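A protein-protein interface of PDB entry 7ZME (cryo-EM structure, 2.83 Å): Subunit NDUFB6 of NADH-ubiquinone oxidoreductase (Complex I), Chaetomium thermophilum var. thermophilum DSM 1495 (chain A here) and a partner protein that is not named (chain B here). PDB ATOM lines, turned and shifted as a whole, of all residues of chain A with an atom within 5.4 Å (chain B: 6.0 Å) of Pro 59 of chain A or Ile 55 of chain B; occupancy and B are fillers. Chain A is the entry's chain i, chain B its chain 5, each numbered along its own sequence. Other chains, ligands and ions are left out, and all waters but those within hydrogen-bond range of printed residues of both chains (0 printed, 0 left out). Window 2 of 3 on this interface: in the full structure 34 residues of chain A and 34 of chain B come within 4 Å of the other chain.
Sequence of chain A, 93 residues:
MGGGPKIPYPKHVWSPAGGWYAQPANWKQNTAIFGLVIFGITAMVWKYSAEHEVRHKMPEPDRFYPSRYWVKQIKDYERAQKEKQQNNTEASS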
ATOM      1  N   ARG A  55       1.062   7.470 -22.582  1.00  0.00           N
ATOM      2  CA  ARG A  55       2.317   8.179 -22.422  1.00  0.00           C
ATOM      3  C   ARG A  55       2.312   8.938 -21.103  1.00  0.00           C
ATOM      4  O   ARG A  55       1.259   9.265 -20.550  1.00  0.00           O
ATOM      5  CB  ARG A  55       2.563   9.155 -23.577  1.00  0.00           C
ATOM      6  CG  ARG A  55       2.471   8.533 -24.953  1.00  0.00           C
ATOM      7  CD  ARG A  55       2.354   9.600 -26.018  1.00  0.00           C
ATOM      8  NE  ARG A  55       2.727   9.119 -27.344  1.00  0.00           N
ATOM      9  CZ  ARG A  55       1.997   8.281 -28.069  1.00  0.00           C
ATOM     10  NH1 ARG A  55       2.414   7.904 -29.269  1.00  0.00           N
ATOM     11  NH2 ARG A  55       0.849   7.816 -27.597  1.00  0.00           N
ATOM     12  N   HIS A  56       3.510   9.207 -20.601  1.00  0.00           N
ATOM     13  CA  HIS A  56       3.688  10.015 -19.412  1.00  0.00           C
ATOM     14  C   HIS A  56       4.385  11.330 -19.703  1.00  0.00           C
ATOM     15  O   HIS A  56       4.598  12.119 -18.775  1.00  0.00           O
ATOM     16  CB  HIS A  56       4.481   9.235 -18.352  1.00  0.00           C
ATOM     17  CG  HIS A  56       3.980   7.843 -18.131  1.00  0.00           C
ATOM     18  ND1 HIS A  56       3.220   7.489 -17.038  1.00  0.00           N
ATOM     19  CD2 HIS A  56       4.124   6.716 -18.869  1.00  0.00           C
ATOM     20  CE1 HIS A  56       2.921   6.205 -17.109  1.00  0.00           C
ATOM     21  NE2 HIS A  56       3.456   5.713 -18.210  1.00  0.00           N
ATOM     22  N   LYS A  57       4.741  11.586 -20.957  1.00  0.00           N
ATOM     23  CA  LYS A  57       5.380  12.816 -21.385  1.00  0.00           C
ATOM     24  C   LYS A  57       4.650  13.333 -22.612  1.00  0.00           C
ATOM     25  O   LYS A  57       4.213  12.549 -23.459  1.00  0.00           O
ATOM     26  CB  LYS A  57       6.860  12.589 -21.704  1.00  0.00           C
ATOM     27  CG  LYS A  57       7.616  13.839 -22.114  1.00  0.00           C
ATOM     28  CD  LYS A  57       7.739  14.815 -20.959  1.00  0.00           C
ATOM     29  CE  LYS A  57       8.484  16.069 -21.379  1.00  0.00           C
ATOM     30  NZ  LYS A  57       9.907  15.782 -21.710  1.00  0.00           N
ATOM     31  N   MET A  58       4.514  14.650 -22.704  1.00  0.00           N
ATOM     32  CA  MET A  58       3.812  15.270 -23.810  1.00  0.00           C
ATOM     33  C   MET A  58       4.809  15.875 -24.782  1.00  0.00           C
ATOM     34  O   MET A  58       5.687  16.641 -24.362  1.00  0.00           O
ATOM     35  CB  MET A  58       2.858  16.353 -23.301  1.00  0.00           C
ATOM     36  CG  MET A  58       1.709  15.839 -22.441  1.00  0.00           C
ATOM     37  SD  MET A  58       0.598  14.697 -23.286  1.00  0.00           S
ATOM     38  CE  MET A  58       1.144  13.122 -22.628  1.00  0.00           C
ATOM     39  N   PRO A  59       4.721  15.555 -26.071  1.00  0.00           N
ATOM     40  CA  PRO A  59       5.652  16.136 -27.040  1.00  0.00           C
ATOM     41  C   PRO A  59       5.475  17.640 -27.167  1.00  0.00           C
ATOM     42  O   PRO A  59       4.381  18.180 -26.981  1.00  0.00           O
ATOM     43  CB  PRO A  59       5.293  15.423 -28.348  1.00  0.00           C
ATOM     44  CG  PRO A  59       3.892  14.968 -28.149  1.00  0.00           C
ATOM     45  CD  PRO A  59       3.780  14.616 -26.704  1.00  0.00           C
ATOM     46  N   GLU A  60       6.574  18.317 -27.488  1.00  0.00           N
ATOM     47  CA  GLU A  60       6.537  19.758 -27.662  1.00  0.00           C
ATOM     48  C   GLU A  60       5.720  20.125 -28.901  1.00  0.00           C
ATOM     49  O   GLU A  60       5.710  19.388 -29.890  1.00  0.00           O
ATOM     50  CB  GLU A  60       7.952  20.318 -27.785  1.00  0.00           C
ATOM     51  CG  GLU A  60       8.780  20.195 -26.517  1.00  0.00           C
ATOM     52  CD  GLU A  60       8.246  21.047 -25.381  1.00  0.00           C
ATOM     53  OE1 GLU A  60       7.567  22.058 -25.659  1.00  0.00           O
ATOM     54  OE2 GLU A  60       8.505  20.704 -24.209  1.00  0.00           O
ATOM     55  N   PRO A  61       5.012  21.258 -28.864  1.00  0.00           N
ATOM     56  CA  PRO A  61       4.185  21.642 -30.020  1.00  0.00           C
ATOM     57  C   PRO A  61       4.977  21.857 -31.298  1.00  0.00           C
ATOM     58  O   PRO A  61       4.459  21.586 -32.389  1.00  0.00           O
ATOM     59  CB  PRO A  61       3.508  22.939 -29.552  1.00  0.00           C
ATOM     60  CG  PRO A  61       3.635  22.935 -28.061  1.00  0.00           C
ATOM     61  CD  PRO A  61       4.918  22.232 -27.765  1.00  0.00           C
ATOM     62  N   TYR A  65       6.121  14.969 -34.650  1.00  0.00           N
ATOM     63  CA  TYR A  65       5.557  13.908 -33.827  1.00  0.00           C
ATOM     64  C   TYR A  65       4.245  13.437 -34.445  1.00  0.00           C
ATOM     65  O   TYR A  65       3.172  13.751 -33.914  1.00  0.00           O
ATOM     66  CB  TYR A  65       5.329  14.416 -32.401  1.00  0.00           C
ATOM     67  CG  TYR A  65       5.315  13.358 -31.324  1.00  0.00           C
ATOM     68  CD1 TYR A  65       6.495  12.889 -30.772  1.00  0.00           C
ATOM     69  CD2 TYR A  65       4.122  12.827 -30.859  1.00  0.00           C
ATOM     70  CE1 TYR A  65       6.489  11.929 -29.787  1.00  0.00           C
ATOM     71  CE2 TYR A  65       4.106  11.866 -29.875  1.00  0.00           C
ATOM     72  CZ  TYR A  65       5.291  11.417 -29.343  1.00  0.00           C
ATOM     73  OH  TYR A  65       5.275  10.454 -28.362  1.00  0.00           O
ATOM     74  N   ARG A  68       0.787  12.677 -32.831  1.00  0.00           N
ATOM     75  CA  ARG A  68      -0.125  13.700 -32.328  1.00  0.00           C
ATOM     76  C   ARG A  68      -1.439  13.749 -33.090  1.00  0.00           C
ATOM     77  O   ARG A  68      -2.432  14.255 -32.556  1.00  0.00           O
ATOM     78  CB  ARG A  68       0.545  15.071 -32.401  1.00  0.00           C
ATOM     79  CG  ARG A  68       1.657  15.289 -31.395  1.00  0.00           C
ATOM     80  CD  ARG A  68       2.085  16.745 -31.374  1.00  0.00           C
ATOM     81  NE  ARG A  68       2.405  17.228 -32.714  1.00  0.00           N
ATOM     82  CZ  ARG A  68       2.684  18.494 -33.005  1.00  0.00           C
ATOM     83  NH1 ARG A  68       2.683  19.412 -32.049  1.00  0.00           N
ATOM     84  NH2 ARG A  68       2.964  18.843 -34.253  1.00  0.00           N
ATOM     85  N   ILE A  74      -2.903  12.175 -26.098  1.00  0.00           N
ATOM     86  CA  ILE A  74      -2.280  13.481 -26.276  1.00  0.00           C
ATOM     87  C   ILE A  74      -3.072  14.385 -27.204  1.00  0.00           C
ATOM     88  O   ILE A  74      -2.804  15.596 -27.237  1.00  0.00           O
ATOM     89  CB  ILE A  74      -0.826  13.357 -26.782  1.00  0.00           C
ATOM     90  CG1 ILE A  74      -0.805  12.934 -28.245  1.00  0.00           C
ATOM     91  CG2 ILE A  74      -0.055  12.351 -25.949  1.00  0.00           C
ATOM     92  CD1 ILE A  74       0.576  12.921 -28.836  1.00  0.00           C
ATOM     93  N   TYR B   2       1.970   1.863 -32.946  1.00  0.00           N
ATOM     94  CA  TYR B   2       2.827   1.031 -32.116  1.00  0.00           C
ATOM     95  C   TYR B   2       2.318  -0.391 -31.969  1.00  0.00           C
ATOM     96  O   TYR B   2       3.083  -1.263 -31.548  1.00  0.00           O
ATOM     97  CB  TYR B   2       2.989   1.660 -30.739  1.00  0.00           C
ATOM     98  CG  TYR B   2       3.872   2.868 -30.765  1.00  0.00           C
ATOM     99  CD1 TYR B   2       5.242   2.742 -30.640  1.00  0.00           C
ATOM    100  CD2 TYR B   2       3.339   4.134 -30.921  1.00  0.00           C
ATOM    101  CE1 TYR B   2       6.054   3.839 -30.667  1.00  0.00           C
ATOM    102  CE2 TYR B   2       4.142   5.239 -30.947  1.00  0.00           C
ATOM    103  CZ  TYR B   2       5.498   5.085 -30.818  1.00  0.00           C
ATOM    104  OH  TYR B   2       6.311   6.181 -30.838  1.00  0.00           O
ATOM    105  N   GLU B  49       9.861   9.432 -32.707  1.00  0.00           N
ATOM    106  CA  GLU B  49       8.857   9.496 -31.653  1.00  0.00           C
ATOM    107  C   GLU B  49       9.468   9.247 -30.279  1.00  0.00           C
ATOM    108  O   GLU B  49       9.460  10.120 -29.407  1.00  0.00           O
ATOM    109  CB  GLU B  49       7.781   8.451 -31.938  1.00  0.00           C
ATOM    110  CG  GLU B  49       6.936   8.660 -33.176  1.00  0.00           C
ATOM    111  CD  GLU B  49       6.046   9.862 -33.088  1.00  0.00           C
ATOM    112  OE1 GLU B  49       5.609  10.180 -31.974  1.00  0.00           O
ATOM    113  OE2 GLU B  49       5.767  10.478 -34.127  1.00  0.00           O
ATOM    114  N   VAL B  50      10.006   8.046 -30.076  1.00  0.00           N
ATOM    115  CA  VAL B  50      10.432   7.627 -28.743  1.00  0.00           C
ATOM    116  C   VAL B  50      11.795   8.209 -28.398  1.00  0.00           C
ATOM    117  O   VAL B  50      11.964   8.879 -27.374  1.00  0.00           O
ATOM    118  CB  VAL B  50      10.441   6.092 -28.638  1.00  0.00           C
ATOM    119  CG1 VAL B  50      10.929   5.672 -27.278  1.00  0.00           C
ATOM    120  CG2 VAL B  50       9.057   5.533 -28.896  1.00  0.00           C
ATOM    121  N   GLY B  51      12.785   7.958 -29.245  1.00  0.00           N
ATOM    122  CA  GLY B  51      14.148   8.311 -28.918  1.00  0.00           C
ATOM    123  C   GLY B  51      14.430   9.796 -28.862  1.00  0.00           C
ATOM    124  O   GLY B  51      14.872  10.309 -27.831  1.00  0.00           O
ATOM    125  N   ASN B  53      12.582  12.277 -28.631  1.00  0.00           N
ATOM    126  CA  ASN B  53      11.715  13.039 -27.749  1.00  0.00           C
ATOM    127  C   ASN B  53      11.698  12.522 -26.322  1.00  0.00           C
ATOM    128  O   ASN B  53      11.122  13.187 -25.453  1.00  0.00           O
ATOM    129  CB  ASN B  53      10.283  13.050 -28.295  1.00  0.00           C
ATOM    130  CG  ASN B  53      10.166  13.814 -29.588  1.00  0.00           C
ATOM    131  OD1 ASN B  53      10.386  15.018 -29.621  1.00  0.00           O
ATOM    132  ND2 ASN B  53       9.811  13.120 -30.661  1.00  0.00           N
ATOM    133  N   ASN B  54      12.310  11.367 -26.058  1.00  0.00           N
ATOM    134  CA  ASN B  54      12.296  10.747 -24.734  1.00  0.00           C
ATOM    135  C   ASN B  54      10.866  10.510 -24.253  1.00  0.00           C
ATOM    136  O   ASN B  54      10.538  10.729 -23.087  1.00  0.00           O
ATOM    137  CB  ASN B  54      13.082  11.584 -23.720  1.00  0.00           C
ATOM    138  CG  ASN B  54      13.378  10.826 -22.441  1.00  0.00           C
ATOM    139  OD1 ASN B  54      13.558   9.610 -22.453  1.00  0.00           O
ATOM    140  ND2 ASN B  54      13.414  11.545 -21.326  1.00  0.00           N
ATOM    141  N   ILE B  55      10.004  10.062 -25.159  1.00  0.00           N
ATOM    142  CA  ILE B  55       8.636   9.716 -24.785  1.00  0.00           C
ATOM    143  C   ILE B  55       8.402   8.235 -25.044  1.00  0.00           C
ATOM    144  O   ILE B  55       7.993   7.859 -26.151  1.00  0.00           O
ATOM    145  CB  ILE B  55       7.600  10.562 -25.540  1.00  0.00           C
ATOM    146  CG1 ILE B  55       7.987  12.037 -25.531  1.00  0.00           C
ATOM    147  CG2 ILE B  55       6.227  10.378 -24.930  1.00  0.00           C
ATOM    148  CD1 ILE B  55       7.199  12.855 -26.507  1.00  0.00           C
ATOM    149  N   PRO B  56       8.644   7.369 -24.067  1.00  0.00           N
ATOM    150  CA  PRO B  56       8.272   5.964 -24.223  1.00  0.00           C
ATOM    151  C   PRO B  56       6.761   5.802 -24.232  1.00  0.00           C
ATOM    152  O   PRO B  56       6.013   6.622 -23.695  1.00  0.00           O
ATOM    153  CB  PRO B  56       8.901   5.287 -23.002  1.00  0.00           C
ATOM    154  CG  PRO B  56       9.058   6.360 -22.011  1.00  0.00           C
ATOM    155  CD  PRO B  56       9.264   7.640 -22.762  1.00  0.00           C
ATOM    156  N   VAL B  57       6.310   4.725 -24.864  1.00  0.00           N
ATOM    157  CA  VAL B  57       4.889   4.449 -25.010  1.00  0.00           C
ATOM    158  C   VAL B  57       4.612   3.024 -24.553  1.00  0.00           C
ATOM    159  O   VAL B  57       5.422   2.119 -24.771  1.00  0.00           O
ATOM    160  CB  VAL B  57       4.412   4.678 -26.459  1.00  0.00           C
ATOM    161  CG1 VAL B  57       5.092   3.723 -27.387  1.00  0.00           C
ATOM    162  CG2 VAL B  57       2.901   4.537 -26.554  1.00  0.00           C
ATOM    163  N   TYR B  78       7.643   0.522 -25.782  1.00  0.00           N
ATOM    164  CA  TYR B  78       8.669   1.075 -26.653  1.00  0.00           C
ATOM    165  C   TYR B  78       9.508   2.054 -25.844  1.00  0.00           C
ATOM    166  O   TYR B  78       8.964   2.949 -25.190  1.00  0.00           O
ATOM    167  CB  TYR B  78       8.060   1.777 -27.863  1.00  0.00           C
ATOM    168  CG  TYR B  78       7.468   0.863 -28.907  1.00  0.00           C
ATOM    169  CD1 TYR B  78       6.352   0.092 -28.633  1.00  0.00           C
ATOM    170  CD2 TYR B  78       8.015   0.791 -30.175  1.00  0.00           C
ATOM    171  CE1 TYR B  78       5.807  -0.733 -29.590  1.00  0.00           C
ATOM    172  CE2 TYR B  78       7.475  -0.027 -31.138  1.00  0.00           C
ATOM    173  CZ  TYR B  78       6.371  -0.787 -30.842  1.00  0.00           C
ATOM    174  OH  TYR B  78       5.832  -1.607 -31.805  1.00  0.00           O
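OH of Tyr 65 of chain A is in hydrogen-bond range of NE of Arg 55 of chain A (3.1 Å). The side-chain hydroxyl of Tyr 78 of chain B is in hydrogen-bond range of the backbone carbonyl oxygen of Tyr 2 of chain B (2.8 Å). ND2 of Asn 53 of chain B lies close to O of Glu 49 of chain B. The backbone NH (N) of Ile 55 of chain B is in hydrogen-bond range of the backbone carbonyl oxygen (O) of Val 50 of chain B, 3.2 Å away.
Hydrophobic or aromatic side chains of chain B within 4 Å of the printed part of chain A: Tyr 2 and Ile 55. Of the 10 printed residues of chain A, 4 touch a printed residue of chain B. Hydrophobic or aromatic side chains of chain A within 4 Å of the printed part of chain B: Pro 59 and Tyr 65. Among the printed residues, 6 pairs touch across the chains.
Among the printed residues, pairs that only touch across the chains: Tyr 65 of chain A with Glu 49 of chain B (2.9 Å), Lys 57 of chain A with Ile 55 of chain B (3.3 Å), Tyr 65 of chain A with Asn 53 of chain B (3.3 Å), Tyr 65 of chain A with Ile 55 of chain B (3.5 Å), Arg 55 of chain A with Tyr 2 of chain B (3.6 Å) and Pro 59 of chain A with Ile 55 of chain B (3.7 Å).
Of the printed residues of chain A, Glu 49 of chain B touches Tyr 65. Of the printed residues of chain B, Lys 57 of chain A touches Ile 55. Of the printed residues of chain B, Tyr 65 of chain A touches Glu 49 (2.9 Å), Asn 53 (3.3 Å) and Ile 55 (3.5 Å). Tyr 78 of chain B touches none of the printed residues of chain A. Asn 54 of chain B touches none of the printed residues of chain A. The nearest residue of chain B that does not touch Pro 59 of chain A is Asn 53 of chain B (5.3 Å).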
